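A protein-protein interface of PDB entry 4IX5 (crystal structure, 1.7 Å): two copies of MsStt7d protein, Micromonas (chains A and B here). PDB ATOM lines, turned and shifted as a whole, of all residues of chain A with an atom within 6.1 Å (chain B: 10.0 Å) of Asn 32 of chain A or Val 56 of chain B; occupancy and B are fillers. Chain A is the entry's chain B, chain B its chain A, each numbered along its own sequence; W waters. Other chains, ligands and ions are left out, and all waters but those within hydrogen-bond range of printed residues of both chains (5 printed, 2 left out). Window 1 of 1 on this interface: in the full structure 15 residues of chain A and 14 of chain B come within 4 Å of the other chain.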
ATOM      1  N   SER A  30      -5.925  -8.252  17.471  1.00  0.00           N
ATOM      2  CA  SER A  30      -7.063  -8.487  18.338  1.00  0.00           C
ATOM      3  C   SER A  30      -7.760  -9.739  17.840  1.00  0.00           C
ATOM      4  O   SER A  30      -8.261  -9.773  16.717  1.00  0.00           O
ATOM      5  CB  SER A  30      -8.021  -7.307  18.267  1.00  0.00           C
ATOM      6  OG  SER A  30      -8.377  -7.049  16.917  1.00  0.00           O
ATOM      7  N   GLY A  31      -7.772 -10.777  18.666  1.00  0.00           N
ATOM      8  CA  GLY A  31      -8.401 -12.025  18.288  1.00  0.00           C
ATOM      9  C   GLY A  31      -9.839 -12.049  18.741  1.00  0.00           C
ATOM     10  O   GLY A  31     -10.476 -11.003  18.871  1.00  0.00           O
ATOM     11  N   ASN A  32     -10.353 -13.245  18.987  1.00  0.00           N
ATOM     12  CA  ASN A  32     -11.734 -13.386  19.410  1.00  0.00           C
ATOM     13  C   ASN A  32     -11.899 -13.096  20.896  1.00  0.00           C
ATOM     14  O   ASN A  32     -12.883 -12.478  21.308  1.00  0.00           O
ATOM     15  CB  ASN A  32     -12.260 -14.781  19.067  1.00  0.00           C
ATOM     16  CG  ASN A  32     -12.471 -14.970  17.572  1.00  0.00           C
ATOM     17  OD1 ASN A  32     -12.671 -14.002  16.837  1.00  0.00           O
ATOM     18  ND2 ASN A  32     -12.427 -16.217  17.116  1.00  0.00           N
ATOM     19  N   PHE A  33     -10.933 -13.530  21.700  1.00  0.00           N
ATOM     20  CA  PHE A  33     -11.082 -13.406  23.138  1.00  0.00           C
ATOM     21  C   PHE A  33      -9.883 -12.771  23.833  1.00  0.00           C
ATOM     22  O   PHE A  33      -9.878 -12.660  25.050  1.00  0.00           O
ATOM     23  CB  PHE A  33     -11.409 -14.762  23.786  1.00  0.00           C
ATOM     24  CG  PHE A  33     -10.301 -15.786  23.669  1.00  0.00           C
ATOM     25  CD1 PHE A  33      -9.261 -15.826  24.599  1.00  0.00           C
ATOM     26  CD2 PHE A  33     -10.309 -16.720  22.644  1.00  0.00           C
ATOM     27  CE1 PHE A  33      -8.247 -16.773  24.494  1.00  0.00           C
ATOM     28  CE2 PHE A  33      -9.298 -17.668  22.536  1.00  0.00           C
ATOM     29  CZ  PHE A  33      -8.268 -17.693  23.462  1.00  0.00           C
ATOM     30  N   GLY A  34      -8.883 -12.350  23.062  1.00  0.00           N
ATOM     31  CA  GLY A  34      -7.651 -11.821  23.644  1.00  0.00           C
ATOM     32  C   GLY A  34      -6.977 -10.756  22.795  1.00  0.00           C
ATOM     33  O   GLY A  34      -7.380 -10.508  21.656  1.00  0.00           O
ATOM     34  N   LYS A  53      -9.570 -10.367  26.584  1.00  0.00           N
ATOM     35  CA  LYS A  53     -10.465  -9.227  26.426  1.00  0.00           C
ATOM     36  C   LYS A  53     -11.455  -9.155  27.587  1.00  0.00           C
ATOM     37  O   LYS A  53     -12.154 -10.129  27.888  1.00  0.00           O
ATOM     38  CB  LYS A  53     -11.209  -9.327  25.096  1.00  0.00           C
ATOM     39  CG  LYS A  53     -10.299  -8.995  23.932  1.00  0.00           C
ATOM     40  CD  LYS A  53     -10.939  -9.373  22.615  1.00  0.00           C
ATOM     41  CE  LYS A  53     -11.394  -8.141  21.867  1.00  0.00           C
ATOM     42  NZ  LYS A  53     -11.894  -8.504  20.517  1.00  0.00           N
ATOM     43  N   VAL A  56     -15.413  -9.923  26.710  1.00  0.00           N
ATOM     44  CA  VAL A  56     -15.870 -11.178  26.123  1.00  0.00           C
ATOM     45  C   VAL A  56     -16.132 -12.245  27.166  1.00  0.00           C
ATOM     46  O   VAL A  56     -15.275 -12.547  27.994  1.00  0.00           O
ATOM     47  CB  VAL A  56     -14.864 -11.686  25.090  1.00  0.00           C
ATOM     48  CG1 VAL A  56     -15.324 -13.021  24.513  1.00  0.00           C
ATOM     49  CG2 VAL A  56     -14.684 -10.636  23.999  1.00  0.00           C
ATOM     50  N   PRO A 210     -15.595 -22.194  17.487  1.00  0.00           N
ATOM     51  CA  PRO A 210     -15.127 -21.087  16.659  1.00  0.00           C
ATOM     52  C   PRO A 210     -14.456 -21.652  15.414  1.00  0.00           C
ATOM     53  O   PRO A 210     -13.954 -22.774  15.439  1.00  0.00           O
ATOM     54  CB  PRO A 210     -14.087 -20.413  17.549  1.00  0.00           C
ATOM     55  CG  PRO A 210     -13.540 -21.533  18.365  1.00  0.00           C
ATOM     56  CD  PRO A 210     -14.703 -22.451  18.630  1.00  0.00           C
ATOM     57  N   ALA A 211     -14.457 -20.890  14.333  1.00  0.00           N
ATOM     58  CA  ALA A 211     -13.755 -21.313  13.138  1.00  0.00           C
ATOM     59  C   ALA A 211     -13.633 -20.137  12.197  1.00  0.00           C
ATOM     60  O   ALA A 211     -14.535 -19.303  12.106  1.00  0.00           O
ATOM     61  CB  ALA A 211     -14.493 -22.456  12.464  1.00  0.00           C
ATOM     62  N   ASP A 212     -12.502 -20.061  11.511  1.00  0.00           N
ATOM     63  CA  ASP A 212     -12.330 -19.092  10.450  1.00  0.00           C
ATOM     64  C   ASP A 212     -13.070 -19.637   9.240  1.00  0.00           C
ATOM     65  O   ASP A 212     -12.680 -20.658   8.679  1.00  0.00           O
ATOM     66  CB  ASP A 212     -10.840 -18.913  10.134  1.00  0.00           C
ATOM     67  CG  ASP A 212     -10.577 -17.749   9.207  1.00  0.00           C
ATOM     68  OD1 ASP A 212     -11.379 -17.550   8.270  1.00  0.00           O
ATOM     69  OD2 ASP A 212      -9.587 -17.021   9.429  1.00  0.00           O
ATOM     70  N   PRO A 213     -14.158 -18.965   8.836  1.00  0.00           N
ATOM     71  CA  PRO A 213     -14.960 -19.524   7.744  1.00  0.00           C
ATOM     72  C   PRO A 213     -14.208 -19.587   6.418  1.00  0.00           C
ATOM     73  O   PRO A 213     -14.701 -20.206   5.482  1.00  0.00           O
ATOM     74  CB  PRO A 213     -16.154 -18.566   7.654  1.00  0.00           C
ATOM     75  CG  PRO A 213     -15.658 -17.277   8.206  1.00  0.00           C
ATOM     76  CD  PRO A 213     -14.612 -17.624   9.247  1.00  0.00           C
ATOM     77  N   SER B  30     -11.851  -3.522  17.687  1.00  0.00           N
ATOM     78  CA  SER B  30     -12.493  -4.650  17.046  1.00  0.00           C
ATOM     79  C   SER B  30     -13.356  -5.334  18.088  1.00  0.00           C
ATOM     80  O   SER B  30     -12.911  -5.591  19.212  1.00  0.00           O
ATOM     81  CB  SER B  30     -11.449  -5.620  16.504  1.00  0.00           C
ATOM     82  OG  SER B  30     -10.627  -6.082  17.558  1.00  0.00           O
ATOM     83  N   GLY B  31     -14.600  -5.600  17.715  1.00  0.00           N
ATOM     84  CA  GLY B  31     -15.532  -6.270  18.595  1.00  0.00           C
ATOM     85  C   GLY B  31     -15.641  -7.714  18.183  1.00  0.00           C
ATOM     86  O   GLY B  31     -14.789  -8.229  17.469  1.00  0.00           O
ATOM     87  N   ASN B  32     -16.704  -8.371  18.619  1.00  0.00           N
ATOM     88  CA  ASN B  32     -16.864  -9.790  18.352  1.00  0.00           C
ATOM     89  C   ASN B  32     -16.766 -10.165  16.869  1.00  0.00           C
ATOM     90  O   ASN B  32     -16.123 -11.161  16.524  1.00  0.00           O
ATOM     91  CB  ASN B  32     -18.155 -10.318  18.988  1.00  0.00           C
ATOM     92  CG  ASN B  32     -18.144 -10.196  20.508  1.00  0.00           C
ATOM     93  OD1 ASN B  32     -17.092  -9.985  21.115  1.00  0.00           O
ATOM     94  ND2 ASN B  32     -19.312 -10.333  21.127  1.00  0.00           N
ATOM     95  N   PHE B  33     -17.370  -9.362  15.994  1.00  0.00           N
ATOM     96  CA  PHE B  33     -17.471  -9.735  14.586  1.00  0.00           C
ATOM     97  C   PHE B  33     -17.057  -8.668  13.578  1.00  0.00           C
ATOM     98  O   PHE B  33     -17.088  -8.924  12.377  1.00  0.00           O
ATOM     99  CB  PHE B  33     -18.888 -10.218  14.259  1.00  0.00           C
ATOM    100  CG  PHE B  33     -19.956  -9.171  14.480  1.00  0.00           C
ATOM    101  CD1 PHE B  33     -20.244  -8.232  13.495  1.00  0.00           C
ATOM    102  CD2 PHE B  33     -20.673  -9.130  15.672  1.00  0.00           C
ATOM    103  CE1 PHE B  33     -21.225  -7.257  13.699  1.00  0.00           C
ATOM    104  CE2 PHE B  33     -21.649  -8.163  15.879  1.00  0.00           C
ATOM    105  CZ  PHE B  33     -21.927  -7.228  14.883  1.00  0.00           C
ATOM    106  N   GLY B  34     -16.663  -7.485  14.039  1.00  0.00           N
ATOM    107  CA  GLY B  34     -16.339  -6.424  13.100  1.00  0.00           C
ATOM    108  C   GLY B  34     -15.208  -5.515  13.535  1.00  0.00           C
ATOM    109  O   GLY B  34     -14.697  -5.637  14.646  1.00  0.00           O
ATOM    110  N   THR B  35     -14.821  -4.601  12.650  1.00  0.00           N
ATOM    111  CA  THR B  35     -13.754  -3.654  12.941  1.00  0.00           C
ATOM    112  C   THR B  35     -14.187  -2.225  12.633  1.00  0.00           C
ATOM    113  O   THR B  35     -14.770  -1.956  11.585  1.00  0.00           O
ATOM    114  CB  THR B  35     -12.489  -3.975  12.139  1.00  0.00           C
ATOM    115  OG1 THR B  35     -12.239  -5.386  12.187  1.00  0.00           O
ATOM    116  CG2 THR B  35     -11.296  -3.214  12.712  1.00  0.00           C
ATOM    117  N   ASN B  51     -16.814  -2.625   9.389  1.00  0.00           N
ATOM    118  CA  ASN B  51     -17.002  -3.721   8.450  1.00  0.00           C
ATOM    119  C   ASN B  51     -16.984  -5.053   9.192  1.00  0.00           C
ATOM    120  O   ASN B  51     -16.789  -5.083  10.401  1.00  0.00           O
ATOM    121  CB  ASN B  51     -15.982  -3.663   7.312  1.00  0.00           C
ATOM    122  CG  ASN B  51     -14.637  -4.216   7.702  1.00  0.00           C
ATOM    123  OD1 ASN B  51     -14.263  -4.201   8.867  1.00  0.00           O
ATOM    124  ND2 ASN B  51     -13.895  -4.716   6.715  1.00  0.00           N
ATOM    125  N   ALA B  52     -17.216  -6.152   8.485  1.00  0.00           N
ATOM    126  CA  ALA B  52     -17.231  -7.469   9.121  1.00  0.00           C
ATOM    127  C   ALA B  52     -15.854  -8.115   9.072  1.00  0.00           C
ATOM    128  O   ALA B  52     -15.144  -7.976   8.080  1.00  0.00           O
ATOM    129  CB  ALA B  52     -18.246  -8.372   8.431  1.00  0.00           C
ATOM    130  N   LYS B  53     -15.493  -8.824  10.139  1.00  0.00           N
ATOM    131  CA  LYS B  53     -14.224  -9.540  10.190  1.00  0.00           C
ATOM    132  C   LYS B  53     -14.264 -10.738   9.258  1.00  0.00           C
ATOM    133  O   LYS B  53     -15.215 -11.527   9.282  1.00  0.00           O
ATOM    134  CB  LYS B  53     -13.947 -10.016  11.606  1.00  0.00           C
ATOM    135  CG  LYS B  53     -13.471  -8.936  12.550  1.00  0.00           C
ATOM    136  CD  LYS B  53     -13.194  -9.555  13.901  1.00  0.00           C
ATOM    137  CE  LYS B  53     -12.534  -8.590  14.843  1.00  0.00           C
ATOM    138  NZ  LYS B  53     -12.185  -9.321  16.091  1.00  0.00           N
ATOM    139  N   ALA B  54     -13.224 -10.887   8.444  1.00  0.00           N
ATOM    140  CA  ALA B  54     -13.174 -11.993   7.499  1.00  0.00           C
ATOM    141  C   ALA B  54     -12.910 -13.325   8.190  1.00  0.00           C
ATOM    142  O   ALA B  54     -13.188 -14.382   7.622  1.00  0.00           O
ATOM    143  CB  ALA B  54     -12.129 -11.738   6.413  1.00  0.00           C
ATOM    144  N   ASP B  55     -12.392 -13.277   9.415  1.00  0.00           N
ATOM    145  CA  ASP B  55     -12.009 -14.494  10.122  1.00  0.00           C
ATOM    146  C   ASP B  55     -13.044 -14.987  11.132  1.00  0.00           C
ATOM    147  O   ASP B  55     -12.789 -15.948  11.863  1.00  0.00           O
ATOM    148  CB  ASP B  55     -10.646 -14.323  10.808  1.00  0.00           C
ATOM    149  CG  ASP B  55     -10.647 -13.214  11.845  1.00  0.00           C
ATOM    150  OD1 ASP B  55     -11.252 -12.153  11.584  1.00  0.00           O
ATOM    151  OD2 ASP B  55     -10.039 -13.401  12.919  1.00  0.00           O
ATOM    152  N   VAL B  56     -14.201 -14.331  11.182  1.00  0.00           N
ATOM    153  CA  VAL B  56     -15.224 -14.689  12.161  1.00  0.00           C
ATOM    154  C   VAL B  56     -16.463 -15.279  11.512  1.00  0.00           C
ATOM    155  O   VAL B  56     -17.013 -14.718  10.562  1.00  0.00           O
ATOM    156  CB  VAL B  56     -15.631 -13.487  13.035  1.00  0.00           C
ATOM    157  CG1 VAL B  56     -16.837 -13.843  13.904  1.00  0.00           C
ATOM    158  CG2 VAL B  56     -14.457 -13.057  13.910  1.00  0.00           C
ATOM    159  N   MET B  57     -16.882 -16.429  12.031  1.00  0.00           N
ATOM    160  CA  MET B  57     -18.056 -17.131  11.554  1.00  0.00           C
ATOM    161  C   MET B  57     -19.262 -16.208  11.628  1.00  0.00           C
ATOM    162  O   MET B  57     -19.482 -15.581  12.649  1.00  0.00           O
ATOM    163  CB  MET B  57     -18.280 -18.361  12.437  1.00  0.00           C
ATOM    164  CG  MET B  57     -19.301 -19.353  11.934  1.00  0.00           C
ATOM    165  SD  MET B  57     -19.473 -20.716  13.115  1.00  0.00           S
ATOM    166  CE  MET B  57     -17.787 -21.302  13.195  1.00  0.00           C
ATOM    167  N   ALA B  58     -19.994 -16.103  10.520  1.00  0.00           N
ATOM    168  CA  ALA B  58     -21.283 -15.405  10.474  1.00  0.00           C
ATOM    169  C   ALA B  58     -21.162 -13.893  10.587  1.00  0.00           C
ATOM    170  O   ALA B  58     -22.151 -13.213  10.859  1.00  0.00           O
ATOM    171  CB  ALA B  58     -22.206 -15.937  11.566  1.00  0.00           C
ATOM    172  N   ALA B  59     -19.960 -13.366  10.382  1.00  0.00           N
ATOM    173  CA  ALA B  59     -19.696 -11.966  10.686  1.00  0.00           C
ATOM    174  C   ALA B  59     -20.562 -11.044   9.853  1.00  0.00           C
ATOM    175  O   ALA B  59     -21.088 -10.060  10.360  1.00  0.00           O
ATOM    176  CB  ALA B  59     -18.216 -11.630  10.508  1.00  0.00           C
ATOM    177  N   GLU B  60     -20.711 -11.366   8.570  1.00  0.00           N
ATOM    178  CA  GLU B  60     -21.508 -10.541   7.675  1.00  0.00           C
ATOM    179  C   GLU B  60     -22.971 -10.515   8.114  1.00  0.00           C
ATOM    180  O   GLU B  60     -23.620  -9.479   8.040  1.00  0.00           O
ATOM    181  CB  GLU B  60     -21.409 -11.046   6.235  1.00  0.00           C
ATOM    182  CG  GLU B  60     -22.203 -10.208   5.243  1.00  0.00           C
ATOM    183  CD  GLU B  60     -22.268 -10.837   3.862  1.00  0.00           C
ATOM    184  OE1 GLU B  60     -22.367 -10.085   2.871  1.00  0.00           O
ATOM    185  OE2 GLU B  60     -22.226 -12.084   3.771  1.00  0.00           O
ATOM    186  N   GLU B  61     -23.473 -11.661   8.568  1.00  0.00           N
ATOM    187  CA  GLU B  61     -24.858 -11.784   9.015  1.00  0.00           C
ATOM    188  C   GLU B  61     -25.072 -11.010  10.311  1.00  0.00           C
ATOM    189  O   GLU B  61     -26.119 -10.384  10.501  1.00  0.00           O
ATOM    190  CB  GLU B  61     -25.239 -13.255   9.214  1.00  0.00           C
ATOM    191  CG  GLU B  61     -25.441 -14.052   7.909  1.00  0.00           C
ATOM    192  CD  GLU B  61     -24.141 -14.355   7.160  1.00  0.00           C
ATOM    193  OE1 GLU B  61     -23.093 -14.574   7.810  1.00  0.00           O
ATOM    194  OE2 GLU B  61     -24.172 -14.378   5.907  1.00  0.00           O
ATOM    195  N   LEU B  62     -24.092 -11.065  11.207  1.00  0.00           N
ATOM    196  CA  LEU B  62     -24.151 -10.293  12.447  1.00  0.00           C
ATOM    197  C   LEU B  62     -24.164  -8.803  12.143  1.00  0.00           C
ATOM    198  O   LEU B  62     -24.929  -8.044  12.747  1.00  0.00           O
ATOM    199  CB  LEU B  62     -22.987 -10.669  13.370  1.00  0.00           C
ATOM    200  CG  LEU B  62     -23.143 -12.090  13.928  1.00  0.00           C
ATOM    201  CD1 LEU B  62     -21.809 -12.642  14.409  1.00  0.00           C
ATOM    202  CD2 LEU B  62     -24.177 -12.089  15.051  1.00  0.00           C
ATOM    203  N   LEU B  63     -23.361  -8.381  11.168  1.00  0.00           N
ATOM    204  CA  LEU B  63     -23.331  -6.965  10.786  1.00  0.00           C
ATOM    205  C   LEU B  63     -24.656  -6.550  10.140  1.00  0.00           C
ATOM    206  O   LEU B  63     -25.128  -5.430  10.334  1.00  0.00           O
ATOM    207  CB  LEU B  63     -22.164  -6.673   9.835  1.00  0.00           C
ATOM    208  CG  LEU B  63     -21.824  -5.203   9.552  1.00  0.00           C
ATOM    209  CD1 LEU B  63     -21.342  -4.480  10.823  1.00  0.00           C
ATOM    210  CD2 LEU B  63     -20.767  -5.110   8.447  1.00  0.00           C
ATOM    211  N   ALA B 211     -22.685 -11.478  25.778  1.00  0.00           N
ATOM    212  CA  ALA B 211     -22.765 -10.569  26.914  1.00  0.00           C
ATOM    213  C   ALA B 211     -21.376 -10.145  27.337  1.00  0.00           C
ATOM    214  O   ALA B 211     -20.405 -10.870  27.149  1.00  0.00           O
ATOM    215  CB  ALA B 211     -23.491 -11.225  28.076  1.00  0.00           C
HETATM  216  O   HOH W   1     -12.440 -17.215  14.370  1.00  0.00           O
HETATM  217  O   HOH W   2     -15.585 -17.764  14.290  1.00  0.00           O
HETATM  218  O   HOH W   3     -14.861  -7.886  21.906  1.00  0.00           O
HETATM  219  O   HOH W   4     -15.395 -12.675  20.581  1.00  0.00           O
HETATM  220  O   HOH W   5     -15.740 -13.415  17.988  1.00  0.00           O
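The side-chain amino group of Lys 53 of chain A is in hydrogen-bond range of the backbone carbonyl oxygen of Ser 30 of chain B, 3.4 Å away.
OG of Ser 30 of chain B is in hydrogen-bond range of OG of Ser 30 of chain A (2.5 Å).
NZ of Lys 53 of chain B lies within hydrogen-bond range of O of Gly 31 of chain B (3.1 Å).
The backbone carbonyl oxygen of Gly 31 of chain A sits at hydrogen-bond distance from the side-chain amino group of Lys 53 of chain A, at 3.3 Å.
The backbone NH (N) of Lys 53 of chain A sits at hydrogen-bond distance from the backbone carbonyl oxygen (O) of Phe 33 of chain A, 2.8 Å away.
The backbone NH (N) of Lys 53 of chain B sits at hydrogen-bond distance from the backbone carbonyl oxygen (O) of Phe 33 of chain B (2.8 Å).
O of Ser 30 of chain A touches NZ of Lys 53 of chain B, at 3.999 Å.
Lys 53 of chain B touches Gly 31 of chain A (NZ to O, 3.7 Å).
Val 56 of chain B touches Asn 32 of chain A.
O of Ala 211 of chain A touches O of Asp 55 of chain B, at 3.8 Å.
Asp 212 of chain A touches Ala 54 of chain B (OD1 to O, 3.7 Å).
CB of Asp 55 of chain B touches OD2 of Asp 212 of chain A, 3.2 Å away.
O of Ala 54 of chain B touches CG of Pro 213 of chain A, 3.9 Å away.
Pro 213 of chain A touches Asp 55 of chain B.
CG of Pro 213 of chain A touches O of Val 56 of chain B, 3.7 Å away.
CD of Pro 213 of chain A touches N of Met 57 of chain B (3.8 Å).
Of chain B, only Val 56 comes within 4 Å of Asn 32 of chain A.
Of the printed residues of chain A, Val 56 of chain B touches Asn 32 (3.6 Å) and Pro 213 (3.7 Å).
Of the printed residues of chain B, Gly 31 of chain A touches Lys 53.
No residue of chain B comes within 4 Å of Gly 34 of chain A.
Of the printed residues of chain B, Val 56 of chain A touches Asn 32 (3.8 Å).
Printed residues of chain B within 4 Å of Lys 53 of chain A: Ser 30.
Of the printed residues of chain A, Ala 54 of chain B touches Asp 212 and Pro 213.
Printed residues of chain B within 4 Å of Ser 30 of chain A: Ser 30 and Lys 53.
Printed residues of chain A within 4 Å of Ser 30 of chain B: Ser 30 (2.5 Å) and Lys 53 (3.4 Å).
The nearest residue of chain B that does not touch Asn 32 of chain A is Asn 32 of chain B (4.5 Å).
The nearest printed residue of chain A that does not touch Asn 32 of chain B is Asn 32 of chain A (4.5 Å).
Along chain B the printed residues that touch a printed residue of chain A span positions 30 to 57.
Of the 11 printed residues of chain A, 8 touch a printed residue of chain B.
Printed residues of chain A that touch a printed residue of chain B: Ser 30, Gly 31, Asn 32, Lys 53, Val 56, Ala 211, Asp 212 and Pro 213.
Among the printed residues, 14 pairs touch across the chains.
Among the printed residues, no Asp or Glu carboxylate lies within 4 Å of a Lys or Arg side-chain nitrogen of the other chain.
Ser 30 of chain B touches its own counterpart, Ser 30 of chain A.
Ser 30 of chain A touches Lys 53 of chain B, and with the chains exchanged Lys 53 of chain A touches Ser 30 of chain B.
Gly 31 of chain A touches Lys 53 of chain B, but with the chains exchanged Lys 53 of chain A does not touch Gly 31 of chain B (4.2 Å).
Asn 32 of chain A touches Val 56 of chain B, and with the chains exchanged Val 56 of chain A touches Asn 32 of chain B.
Of the 14 pairs that touch across the chains among the printed residues, 5 have their exchanged pair printed and touching as well.
Water W4 lies within hydrogen-bond range of the backbone carbonyl oxygen of Asn 32 of chain A (2.6 Å) and the side-chain amide oxygen of Asn 32 of chain B (3.2 Å).
Water W5 bridges O of Asn 32 of chain B (2.7 Å) and OD1 of Asn 32 of chain A (3.3 Å).
Water W1 bridges the backbone carbonyl oxygen (O) of Asp 55 of chain B (2.8 Å) and the side-chain amide nitrogen (ND2) of Asn 32 of chain A (2.9 Å).
Water W2 lies within hydrogen-bond range of O of Ala 211 of chain A (2.9 Å) and N of Met 57 of chain B (2.9 Å).
Water W3 lies within hydrogen-bond range of the side-chain amide oxygen (OD1) of Asn 32 of chain B and the side-chain amino group (NZ) of Lys 53 of chain A.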
